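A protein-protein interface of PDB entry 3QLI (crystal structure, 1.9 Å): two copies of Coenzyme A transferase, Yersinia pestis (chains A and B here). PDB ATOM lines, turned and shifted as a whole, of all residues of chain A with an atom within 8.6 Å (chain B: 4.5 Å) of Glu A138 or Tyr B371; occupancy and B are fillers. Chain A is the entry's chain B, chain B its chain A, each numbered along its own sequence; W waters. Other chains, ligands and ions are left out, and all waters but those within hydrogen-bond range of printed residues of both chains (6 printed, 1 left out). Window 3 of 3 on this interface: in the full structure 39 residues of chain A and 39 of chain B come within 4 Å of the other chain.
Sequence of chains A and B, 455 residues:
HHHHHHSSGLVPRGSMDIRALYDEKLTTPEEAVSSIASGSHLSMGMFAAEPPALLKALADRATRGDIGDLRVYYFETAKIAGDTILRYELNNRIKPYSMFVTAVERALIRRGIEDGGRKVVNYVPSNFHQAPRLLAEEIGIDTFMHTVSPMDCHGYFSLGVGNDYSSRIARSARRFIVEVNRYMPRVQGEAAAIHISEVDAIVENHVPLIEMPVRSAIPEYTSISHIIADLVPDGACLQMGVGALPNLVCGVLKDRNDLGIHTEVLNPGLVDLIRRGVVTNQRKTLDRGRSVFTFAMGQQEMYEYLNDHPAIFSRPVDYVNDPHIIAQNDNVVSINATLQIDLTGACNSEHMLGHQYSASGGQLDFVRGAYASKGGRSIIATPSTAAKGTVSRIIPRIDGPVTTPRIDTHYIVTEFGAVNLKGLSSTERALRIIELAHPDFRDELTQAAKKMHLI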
ATOM      1  N   HIS A  41     -29.162   5.052 -29.149  1.00  0.00           N
ATOM      2  CA  HIS A  41     -27.794   5.493 -29.436  1.00  0.00           C
ATOM      3  C   HIS A  41     -26.844   4.499 -28.785  1.00  0.00           C
ATOM      4  O   HIS A  41     -26.998   4.176 -27.612  1.00  0.00           O
ATOM      5  CB  HIS A  41     -27.516   6.878 -28.830  1.00  0.00           C
ATOM      6  CG  HIS A  41     -28.326   7.994 -29.422  1.00  0.00           C
ATOM      7  ND1 HIS A  41     -28.258   9.285 -28.943  1.00  0.00           N
ATOM      8  CD2 HIS A  41     -29.204   8.020 -30.455  1.00  0.00           C
ATOM      9  CE1 HIS A  41     -29.059  10.061 -29.656  1.00  0.00           C
ATOM     10  NE2 HIS A  41     -29.638   9.320 -30.585  1.00  0.00           N
ATOM     11  N   TYR A  73     -22.237   6.003 -32.469  1.00  0.00           N
ATOM     12  CA  TYR A  73     -21.315   7.118 -32.338  1.00  0.00           C
ATOM     13  C   TYR A  73     -19.989   6.559 -31.832  1.00  0.00           C
ATOM     14  O   TYR A  73     -19.957   5.873 -30.803  1.00  0.00           O
ATOM     15  CB  TYR A  73     -21.853   8.104 -31.305  1.00  0.00           C
ATOM     16  CG  TYR A  73     -23.091   8.890 -31.690  1.00  0.00           C
ATOM     17  CD1 TYR A  73     -22.983  10.205 -32.145  1.00  0.00           C
ATOM     18  CD2 TYR A  73     -24.374   8.350 -31.535  1.00  0.00           C
ATOM     19  CE1 TYR A  73     -24.114  10.960 -32.460  1.00  0.00           C
ATOM     20  CE2 TYR A  73     -25.515   9.097 -31.854  1.00  0.00           C
ATOM     21  CZ  TYR A  73     -25.374  10.404 -32.321  1.00  0.00           C
ATOM     22  OH  TYR A  73     -26.489  11.161 -32.645  1.00  0.00           O
ATOM     23  N   MET A  99     -17.196   9.877 -35.690  1.00  0.00           N
ATOM     24  CA  MET A  99     -16.642  11.097 -35.122  1.00  0.00           C
ATOM     25  C   MET A  99     -15.191  11.355 -35.546  1.00  0.00           C
ATOM     26  O   MET A  99     -14.680  12.461 -35.371  1.00  0.00           O
ATOM     27  CB  MET A  99     -16.875  11.130 -33.613  1.00  0.00           C
ATOM     28  CG  MET A  99     -18.373  11.092 -33.306  1.00  0.00           C
ATOM     29  SD  MET A  99     -18.828  10.952 -31.577  1.00  0.00           S
ATOM     30  CE  MET A  99     -18.574  12.644 -31.028  1.00  0.00           C
ATOM     31  N   VAL A 124     -20.023  13.608 -37.238  1.00  0.00           N
ATOM     32  CA  VAL A 124     -20.395  14.486 -36.137  1.00  0.00           C
ATOM     33  C   VAL A 124     -19.162  15.313 -35.752  1.00  0.00           C
ATOM     34  O   VAL A 124     -18.218  14.781 -35.155  1.00  0.00           O
ATOM     35  CB  VAL A 124     -20.847  13.681 -34.912  1.00  0.00           C
ATOM     36  CG1 VAL A 124     -21.196  14.614 -33.757  1.00  0.00           C
ATOM     37  CG2 VAL A 124     -22.039  12.796 -35.254  1.00  0.00           C
ATOM     38  N   SER A 126     -16.611  17.512 -33.800  1.00  0.00           N
ATOM     39  CA  SER A 126     -16.366  17.639 -32.378  1.00  0.00           C
ATOM     40  C   SER A 126     -14.882  17.755 -32.114  1.00  0.00           C
ATOM     41  O   SER A 126     -14.075  17.542 -33.001  1.00  0.00           O
ATOM     42  CB  SER A 126     -16.898  16.420 -31.622  1.00  0.00           C
ATOM     43  OG  SER A 126     -16.009  15.320 -31.744  1.00  0.00           O
ATOM     44  N   ASN A 127     -14.539  18.076 -30.877  1.00  0.00           N
ATOM     45  CA  ASN A 127     -13.170  17.944 -30.424  1.00  0.00           C
ATOM     46  C   ASN A 127     -13.042  16.644 -29.661  1.00  0.00           C
ATOM     47  O   ASN A 127     -13.793  16.404 -28.728  1.00  0.00           O
ATOM     48  CB  ASN A 127     -12.813  19.098 -29.504  1.00  0.00           C
ATOM     49  CG  ASN A 127     -12.635  20.385 -30.256  1.00  0.00           C
ATOM     50  OD1 ASN A 127     -11.720  20.508 -31.059  1.00  0.00           O
ATOM     51  ND2 ASN A 127     -13.505  21.349 -30.008  1.00  0.00           N
ATOM     52  N   HIS A 129     -11.074  15.912 -27.493  1.00  0.00           N
ATOM     53  CA  HIS A 129     -10.821  16.210 -26.082  1.00  0.00           C
ATOM     54  C   HIS A 129     -12.107  16.447 -25.290  1.00  0.00           C
ATOM     55  O   HIS A 129     -12.089  16.436 -24.063  1.00  0.00           O
ATOM     56  CB  HIS A 129      -9.817  17.377 -25.891  1.00  0.00           C
ATOM     57  CG  HIS A 129     -10.352  18.727 -26.287  1.00  0.00           C
ATOM     58  ND1 HIS A 129      -9.729  19.532 -27.218  1.00  0.00           N
ATOM     59  CD2 HIS A 129     -11.430  19.424 -25.854  1.00  0.00           C
ATOM     60  CE1 HIS A 129     -10.408  20.659 -27.353  1.00  0.00           C
ATOM     61  NE2 HIS A 129     -11.450  20.616 -26.542  1.00  0.00           N
ATOM     62  N   GLN A 130     -13.217  16.656 -25.997  1.00  0.00           N
ATOM     63  CA  GLN A 130     -14.509  16.906 -25.359  1.00  0.00           C
ATOM     64  C   GLN A 130     -15.439  15.700 -25.483  1.00  0.00           C
ATOM     65  O   GLN A 130     -16.589  15.761 -25.049  1.00  0.00           O
ATOM     66  CB  GLN A 130     -15.200  18.131 -25.994  1.00  0.00           C
ATOM     67  CG  GLN A 130     -14.458  19.432 -25.753  1.00  0.00           C
ATOM     68  CD  GLN A 130     -14.999  20.609 -26.551  1.00  0.00           C
ATOM     69  OE1 GLN A 130     -15.675  20.443 -27.560  1.00  0.00           O
ATOM     70  NE2 GLN A 130     -14.676  21.806 -26.105  1.00  0.00           N
ATOM     71  N   ALA A 131     -14.941  14.613 -26.068  1.00  0.00           N
ATOM     72  CA  ALA A 131     -15.786  13.437 -26.356  1.00  0.00           C
ATOM     73  C   ALA A 131     -16.572  12.871 -25.173  1.00  0.00           C
ATOM     74  O   ALA A 131     -17.720  12.476 -25.343  1.00  0.00           O
ATOM     75  CB  ALA A 131     -14.975  12.341 -27.017  1.00  0.00           C
ATOM     76  N   PRO A 132     -15.956  12.801 -23.977  1.00  0.00           N
ATOM     77  CA  PRO A 132     -16.687  12.228 -22.841  1.00  0.00           C
ATOM     78  C   PRO A 132     -17.941  13.049 -22.536  1.00  0.00           C
ATOM     79  O   PRO A 132     -19.045  12.520 -22.447  1.00  0.00           O
ATOM     80  CB  PRO A 132     -15.673  12.310 -21.698  1.00  0.00           C
ATOM     81  CG  PRO A 132     -14.316  12.286 -22.407  1.00  0.00           C
ATOM     82  CD  PRO A 132     -14.569  13.147 -23.622  1.00  0.00           C
ATOM     83  N   ARG A 133     -17.787  14.354 -22.425  1.00  0.00           N
ATOM     84  CA  ARG A 133     -18.961  15.190 -22.208  1.00  0.00           C
ATOM     85  C   ARG A 133     -19.942  15.174 -23.380  1.00  0.00           C
ATOM     86  O   ARG A 133     -21.155  15.071 -23.178  1.00  0.00           O
ATOM     87  CB  ARG A 133     -18.549  16.626 -21.902  1.00  0.00           C
ATOM     88  CG  ARG A 133     -19.724  17.560 -21.915  1.00  0.00           C
ATOM     89  CD  ARG A 133     -19.303  18.995 -21.776  1.00  0.00           C
ATOM     90  NE  ARG A 133     -20.466  19.875 -21.828  1.00  0.00           N
ATOM     91  CZ  ARG A 133     -20.376  21.192 -21.717  1.00  0.00           C
ATOM     92  NH1 ARG A 133     -19.174  21.738 -21.554  1.00  0.00           N
ATOM     93  NH2 ARG A 133     -21.471  21.950 -21.767  1.00  0.00           N
ATOM     94  N   LEU A 134     -19.434  15.275 -24.605  1.00  0.00           N
ATOM     95  CA  LEU A 134     -20.309  15.295 -25.777  1.00  0.00           C
ATOM     96  C   LEU A 134     -21.198  14.053 -25.844  1.00  0.00           C
ATOM     97  O   LEU A 134     -22.422  14.152 -26.013  1.00  0.00           O
ATOM     98  CB  LEU A 134     -19.493  15.411 -27.062  1.00  0.00           C
ATOM     99  CG  LEU A 134     -20.196  16.193 -28.173  1.00  0.00           C
ATOM    100  CD1 LEU A 134     -20.310  17.677 -27.793  1.00  0.00           C
ATOM    101  CD2 LEU A 134     -19.476  16.034 -29.495  1.00  0.00           C
ATOM    102  N   LEU A 135     -20.585  12.881 -25.710  1.00  0.00           N
ATOM    103  CA  LEU A 135     -21.342  11.635 -25.793  1.00  0.00           C
ATOM    104  C   LEU A 135     -22.301  11.434 -24.618  1.00  0.00           C
ATOM    105  O   LEU A 135     -23.439  10.999 -24.805  1.00  0.00           O
ATOM    106  CB  LEU A 135     -20.398  10.434 -25.922  1.00  0.00           C
ATOM    107  CG  LEU A 135     -19.609  10.357 -27.235  1.00  0.00           C
ATOM    108  CD1 LEU A 135     -18.364   9.466 -27.090  1.00  0.00           C
ATOM    109  CD2 LEU A 135     -20.476   9.857 -28.371  1.00  0.00           C
ATOM    110  N   ALA A 136     -21.847  11.737 -23.409  1.00  0.00           N
ATOM    111  CA  ALA A 136     -22.678  11.535 -22.220  1.00  0.00           C
ATOM    112  C   ALA A 136     -23.786  12.571 -22.093  1.00  0.00           C
ATOM    113  O   ALA A 136     -24.908  12.241 -21.706  1.00  0.00           O
ATOM    114  CB  ALA A 136     -21.818  11.535 -20.945  1.00  0.00           C
ATOM    115  N   GLU A 137     -23.474  13.825 -22.409  1.00  0.00           N
ATOM    116  CA  GLU A 137     -24.371  14.929 -22.072  1.00  0.00           C
ATOM    117  C   GLU A 137     -25.122  15.564 -23.241  1.00  0.00           C
ATOM    118  O   GLU A 137     -26.286  15.919 -23.088  1.00  0.00           O
ATOM    119  CB  GLU A 137     -23.636  16.008 -21.273  1.00  0.00           C
ATOM    120  CG  GLU A 137     -23.063  15.492 -19.955  1.00  0.00           C
ATOM    121  CD  GLU A 137     -22.377  16.576 -19.145  1.00  0.00           C
ATOM    122  OE1 GLU A 137     -22.551  17.774 -19.465  1.00  0.00           O
ATOM    123  OE2 GLU A 137     -21.655  16.228 -18.186  1.00  0.00           O
ATOM    124  N   GLU A 138     -24.468  15.729 -24.388  1.00  0.00           N
ATOM    125  CA  GLU A 138     -25.109  16.372 -25.537  1.00  0.00           C
ATOM    126  C   GLU A 138     -25.838  15.332 -26.386  1.00  0.00           C
ATOM    127  O   GLU A 138     -26.976  15.526 -26.791  1.00  0.00           O
ATOM    128  CB  GLU A 138     -24.083  17.106 -26.408  1.00  0.00           C
ATOM    129  CG  GLU A 138     -23.204  18.113 -25.662  1.00  0.00           C
ATOM    130  CD  GLU A 138     -23.852  19.475 -25.540  1.00  0.00           C
ATOM    131  OE1 GLU A 138     -25.028  19.623 -25.955  1.00  0.00           O
ATOM    132  OE2 GLU A 138     -23.180  20.396 -25.033  1.00  0.00           O
ATOM    133  N   ILE A 139     -25.156  14.228 -26.654  1.00  0.00           N
ATOM    134  CA  ILE A 139     -25.674  13.195 -27.534  1.00  0.00           C
ATOM    135  C   ILE A 139     -26.525  12.199 -26.769  1.00  0.00           C
ATOM    136  O   ILE A 139     -27.674  11.947 -27.140  1.00  0.00           O
ATOM    137  CB  ILE A 139     -24.522  12.482 -28.269  1.00  0.00           C
ATOM    138  CG1 ILE A 139     -23.845  13.445 -29.246  1.00  0.00           C
ATOM    139  CG2 ILE A 139     -25.018  11.240 -29.015  1.00  0.00           C
ATOM    140  CD1 ILE A 139     -22.423  13.024 -29.641  1.00  0.00           C
ATOM    141  N   GLY A 140     -25.966  11.642 -25.696  1.00  0.00           N
ATOM    142  CA  GLY A 140     -26.656  10.632 -24.911  1.00  0.00           C
ATOM    143  C   GLY A 140     -26.449   9.256 -25.516  1.00  0.00           C
ATOM    144  O   GLY A 140     -26.819   9.020 -26.664  1.00  0.00           O
ATOM    145  N   ILE A 141     -25.833   8.356 -24.752  1.00  0.00           N
ATOM    146  CA  ILE A 141     -25.572   6.994 -25.205  1.00  0.00           C
ATOM    147  C   ILE A 141     -26.321   5.989 -24.328  1.00  0.00           C
ATOM    148  O   ILE A 141     -26.168   5.983 -23.100  1.00  0.00           O
ATOM    149  CB  ILE A 141     -24.054   6.666 -25.159  1.00  0.00           C
ATOM    150  CG1 ILE A 141     -23.259   7.634 -26.047  1.00  0.00           C
ATOM    151  CG2 ILE A 141     -23.785   5.216 -25.537  1.00  0.00           C
ATOM    152  CD1 ILE A 141     -23.557   7.572 -27.564  1.00  0.00           C
ATOM    153  N   ARG A 168     -15.734   7.079 -19.208  1.00  0.00           N
ATOM    154  CA  ARG A 168     -16.940   7.859 -18.940  1.00  0.00           C
ATOM    155  C   ARG A 168     -18.273   7.288 -19.457  1.00  0.00           C
ATOM    156  O   ARG A 168     -19.281   7.335 -18.755  1.00  0.00           O
ATOM    157  CB  ARG A 168     -16.770   9.293 -19.452  1.00  0.00           C
ATOM    158  CG  ARG A 168     -18.047  10.115 -19.415  1.00  0.00           C
ATOM    159  CD  ARG A 168     -18.196  10.836 -18.089  1.00  0.00           C
ATOM    160  NE  ARG A 168     -19.475  11.531 -17.980  1.00  0.00           N
ATOM    161  CZ  ARG A 168     -19.660  12.812 -18.282  1.00  0.00           C
ATOM    162  NH1 ARG A 168     -18.647  13.548 -18.714  1.00  0.00           N
ATOM    163  NH2 ARG A 168     -20.860  13.358 -18.150  1.00  0.00           N
ATOM    164  N   ILE A 169     -18.276   6.761 -20.680  1.00  0.00           N
ATOM    165  CA  ILE A 169     -19.513   6.280 -21.308  1.00  0.00           C
ATOM    166  C   ILE A 169     -19.880   4.896 -20.792  1.00  0.00           C
ATOM    167  O   ILE A 169     -21.058   4.535 -20.748  1.00  0.00           O
ATOM    168  CB  ILE A 169     -19.414   6.297 -22.846  1.00  0.00           C
ATOM    169  CG1 ILE A 169     -18.933   7.686 -23.307  1.00  0.00           C
ATOM    170  CG2 ILE A 169     -20.763   5.951 -23.484  1.00  0.00           C
ATOM    171  CD1 ILE A 169     -19.760   8.836 -22.721  1.00  0.00           C
ATOM    172  N   VAL B 367     -15.068  31.394 -27.020  1.00  0.00           N
ATOM    173  CA  VAL B 367     -15.905  30.287 -27.496  1.00  0.00           C
ATOM    174  C   VAL B 367     -15.518  29.013 -26.733  1.00  0.00           C
ATOM    175  O   VAL B 367     -16.376  28.284 -26.219  1.00  0.00           O
ATOM    176  CB  VAL B 367     -15.737  30.073 -29.034  1.00  0.00           C
ATOM    177  CG1 VAL B 367     -16.380  28.757 -29.484  1.00  0.00           C
ATOM    178  CG2 VAL B 367     -16.319  31.250 -29.810  1.00  0.00           C
ATOM    179  N   ARG B 368     -14.216  28.753 -26.649  1.00  0.00           N
ATOM    180  CA  ARG B 368     -13.704  27.583 -25.934  1.00  0.00           C
ATOM    181  C   ARG B 368     -13.924  27.679 -24.428  1.00  0.00           C
ATOM    182  O   ARG B 368     -14.351  26.723 -23.786  1.00  0.00           O
ATOM    183  CB  ARG B 368     -12.204  27.431 -26.201  1.00  0.00           C
ATOM    184  CG  ARG B 368     -11.835  27.090 -27.638  1.00  0.00           C
ATOM    185  CD  ARG B 368     -10.312  27.305 -27.841  1.00  0.00           C
ATOM    186  NE  ARG B 368      -9.772  26.625 -29.016  1.00  0.00           N
ATOM    187  CZ  ARG B 368      -8.594  26.919 -29.576  1.00  0.00           C
ATOM    188  NH1 ARG B 368      -7.854  27.902 -29.075  1.00  0.00           N
ATOM    189  NH2 ARG B 368      -8.153  26.242 -30.640  1.00  0.00           N
ATOM    190  N   GLY B 369     -13.589  28.826 -23.852  1.00  0.00           N
ATOM    191  CA  GLY B 369     -13.690  29.006 -22.417  1.00  0.00           C
ATOM    192  C   GLY B 369     -15.123  28.952 -21.913  1.00  0.00           C
ATOM    193  O   GLY B 369     -15.397  28.331 -20.883  1.00  0.00           O
ATOM    194  N   ALA B 370     -16.045  29.588 -22.637  1.00  0.00           N
ATOM    195  CA  ALA B 370     -17.446  29.596 -22.215  1.00  0.00           C
ATOM    196  C   ALA B 370     -18.026  28.179 -22.229  1.00  0.00           C
ATOM    197  O   ALA B 370     -18.742  27.795 -21.315  1.00  0.00           O
ATOM    198  CB  ALA B 370     -18.285  30.539 -23.092  1.00  0.00           C
ATOM    199  N   TYR B 371     -17.700  27.394 -23.250  1.00  0.00           N
ATOM    200  CA  TYR B 371     -18.212  26.021 -23.309  1.00  0.00           C
ATOM    201  C   TYR B 371     -17.677  25.183 -22.145  1.00  0.00           C
ATOM    202  O   TYR B 371     -18.401  24.365 -21.576  1.00  0.00           O
ATOM    203  CB  TYR B 371     -17.894  25.351 -24.650  1.00  0.00           C
ATOM    204  CG  TYR B 371     -18.550  23.991 -24.797  1.00  0.00           C
ATOM    205  CD1 TYR B 371     -19.931  23.877 -24.896  1.00  0.00           C
ATOM    206  CD2 TYR B 371     -17.789  22.825 -24.845  1.00  0.00           C
ATOM    207  CE1 TYR B 371     -20.550  22.629 -25.020  1.00  0.00           C
ATOM    208  CE2 TYR B 371     -18.389  21.579 -24.972  1.00  0.00           C
ATOM    209  CZ  TYR B 371     -19.771  21.489 -25.062  1.00  0.00           C
ATOM    210  OH  TYR B 371     -20.378  20.257 -25.181  1.00  0.00           O
ATOM    211  N   ALA B 372     -16.409  25.390 -21.789  1.00  0.00           N
ATOM    212  CA  ALA B 372     -15.781  24.637 -20.697  1.00  0.00           C
ATOM    213  C   ALA B 372     -16.335  25.009 -19.313  1.00  0.00           C
ATOM    214  O   ALA B 372     -16.276  24.215 -18.370  1.00  0.00           O
ATOM    215  CB  ALA B 372     -14.250  24.821 -20.732  1.00  0.00           C
ATOM    216  N   SER B 373     -16.841  26.235 -19.189  1.00  0.00           N
ATOM    217  CA  SER B 373     -17.410  26.718 -17.939  1.00  0.00           C
ATOM    218  C   SER B 373     -18.602  25.858 -17.529  1.00  0.00           C
ATOM    219  O   SER B 373     -19.426  25.489 -18.368  1.00  0.00           O
ATOM    220  CB  SER B 373     -17.894  28.160 -18.123  1.00  0.00           C
ATOM    221  OG  SER B 373     -18.671  28.582 -17.018  1.00  0.00           O
ATOM    222  N   HIS B 410     -20.669  26.670 -30.570  1.00  0.00           N
ATOM    223  CA  HIS B 410     -21.615  26.186 -29.581  1.00  0.00           C
ATOM    224  C   HIS B 410     -23.023  26.616 -29.953  1.00  0.00           C
ATOM    225  O   HIS B 410     -23.809  25.831 -30.473  1.00  0.00           O
ATOM    226  CB  HIS B 410     -21.252  26.747 -28.204  1.00  0.00           C
ATOM    227  CG  HIS B 410     -22.036  26.152 -27.078  1.00  0.00           C
ATOM    228  ND1 HIS B 410     -22.063  26.707 -25.816  1.00  0.00           N
ATOM    229  CD2 HIS B 410     -22.822  25.051 -27.020  1.00  0.00           C
ATOM    230  CE1 HIS B 410     -22.829  25.973 -25.031  1.00  0.00           C
ATOM    231  NE2 HIS B 410     -23.303  24.963 -25.737  1.00  0.00           N
ATOM    232  N   ASN B 420     -28.026  25.295 -30.837  1.00  0.00           N
ATOM    233  CA  ASN B 420     -26.856  24.710 -30.189  1.00  0.00           C
ATOM    234  C   ASN B 420     -26.332  23.585 -31.082  1.00  0.00           C
ATOM    235  O   ASN B 420     -27.012  22.573 -31.279  1.00  0.00           O
ATOM    236  CB  ASN B 420     -27.261  24.175 -28.811  1.00  0.00           C
ATOM    237  CG  ASN B 420     -26.136  23.439 -28.093  1.00  0.00           C
ATOM    238  OD1 ASN B 420     -25.023  23.289 -28.605  1.00  0.00           O
ATOM    239  ND2 ASN B 420     -26.437  22.967 -26.893  1.00  0.00           N
ATOM    240  N   LYS B 422     -23.559  21.642 -30.769  1.00  0.00           N
ATOM    241  CA  LYS B 422     -22.744  20.575 -30.175  1.00  0.00           C
ATOM    242  C   LYS B 422     -23.410  19.199 -30.211  1.00  0.00           C
ATOM    243  O   LYS B 422     -24.545  19.030 -29.760  1.00  0.00           O
ATOM    244  CB  LYS B 422     -22.338  20.922 -28.743  1.00  0.00           C
ATOM    245  CG  LYS B 422     -21.361  22.104 -28.631  1.00  0.00           C
ATOM    246  CD  LYS B 422     -19.956  21.689 -29.066  1.00  0.00           C
ATOM    247  CE  LYS B 422     -18.960  22.784 -28.784  1.00  0.00           C
ATOM    248  NZ  LYS B 422     -17.608  22.381 -29.296  1.00  0.00           N
ATOM    249  N   GLY B 423     -22.701  18.216 -30.755  1.00  0.00           N
ATOM    250  CA  GLY B 423     -23.194  16.846 -30.788  1.00  0.00           C
ATOM    251  C   GLY B 423     -24.072  16.511 -31.985  1.00  0.00           C
ATOM    252  O   GLY B 423     -24.449  15.354 -32.167  1.00  0.00           O
HETATM  253  O   HOH W   1     -21.137  24.638 -21.035  1.00  0.00           O
HETATM  254  O   HOH W   2     -24.584  22.615 -24.473  1.00  0.00           O
HETATM  255  O   HOH W   3     -13.807  24.219 -24.542  1.00  0.00           O
HETATM  256  O   HOH W   4     -17.089  19.221 -29.109  1.00  0.00           O
HETATM  257  O   HOH W   5     -26.272  13.640 -33.282  1.00  0.00           O
HETATM  258  O   HOH W   6     -21.782  23.092 -18.750  1.00  0.00           O
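Of chain B, only Tyr B371 (2.8 Å), Asn B420 (3.7 Å) and Lys B422 (3.8 Å) come within 4 Å of Glu A138. No residue of chain A comes within 4 Å of Gly B369. Of the printed residues of chain B, Leu A134 touches Tyr B371, Lys B422 and Gly B423. Of the printed residues of chain B, Arg A133 touches Tyr B371 (2.7 Å). Printed residues of chain A within 4 Å of Asn B420: Glu A138. Tyr A73 touches none of the printed residues of chain B. The nearest printed residue of chain B that does not touch Glu A138 is Gly B423 (4.5 Å). The nearest residue of chain A that does not touch Tyr B371 is Glu A137 (6.6 Å). The nearest printed residue of chain A that does not touch Gly B423 is Tyr A73 (4.4 Å).
Water W4 lies within hydrogen-bond range of the side-chain amide oxygen of Gln A130, the side-chain amino group of Lys B422 and the backbone NH of Asn A127. Water W5 lies within hydrogen-bond range of OH of Tyr A73 (2.6 Å) and O of Gly B423 (2.7 Å). Water W3 lies within hydrogen-bond range of O of Arg B368 (2.7 Å) and NE2 of Gln A130 (3.0 Å). Water W2 lies within hydrogen-bond range of the side-chain carboxylate (OE2) of Glu A138 (2.7 Å), a ring nitrogen (NE2) of His B410 (3.0 Å) and the side-chain amide nitrogen (ND2) of Asn B420 (3.1 Å). Water W1 lies within hydrogen-bond range of the backbone carbonyl oxygen of Tyr B371 (2.8 Å), the guanidinium group of Arg A133 (2.8 Å) and the backbone carbonyl oxygen of Ser B373 (3.3 Å). Water W6 lies within hydrogen-bond range of the guanidinium group of Arg A133 (3.2 Å) and the backbone carbonyl oxygen of Ser B373 (3.4 Å).
The backbone NH (N) of Lys B422 is in hydrogen-bond range of the side-chain amide oxygen (OD1) of Asn B420 (3.1 Å). ND1 of His A41 lies within hydrogen-bond range of O of Ile A139 (3.3 Å). The side-chain amide nitrogen (ND2) of Asn A127 sits at hydrogen-bond distance from the side-chain amide oxygen (OE1) of Gln A130. NE2 of His A129 sits close to NE2 of Gln A130, at 3.5 Å. NE of Arg A133 lies within salt-bridge range of OE1 of Glu A137, 3.8 Å away. The backbone NH of Ile A139 lies within hydrogen-bond range of the backbone carbonyl oxygen of Leu A134 (2.8 Å).
Val A124 touches Gly B423 (CG1 to O, 3.7 Å). CD2 of Tyr B371 touches NE2 of Gln A130, 3.5 Å away. Leu A134 touches Tyr B371. Leu A134 touches Lys B422 (CD1 to CB, 3.9 Å). CD1 of Leu A134 touches N of Gly B423, 3.8 Å away. Asn B420 touches Glu A138. Lys B422 touches Glu A138. Ile A139 touches Gly B423.
Of the 11 printed residues of chain B, 4 touch a printed residue of chain A. Among the printed residues, no Asp or Glu carboxylate lies within 4 Å of a Lys or Arg side-chain nitrogen of the other chain.
O of Tyr B371 sits at hydrogen-bond distance from NH1 of Arg A133 (2.7 Å). OH of Tyr B371 is in hydrogen-bond range of OE2 of Glu A138 (2.8 Å). The side-chain amino group (NZ) of Lys B422 is in hydrogen-bond range of the side-chain amide oxygen (OE1) of Gln A130 (3.2 Å).
No position is printed for both chains. Of the 11 pairs that touch across the chains among the printed residues, none has its exchanged pair printed and touching as well.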
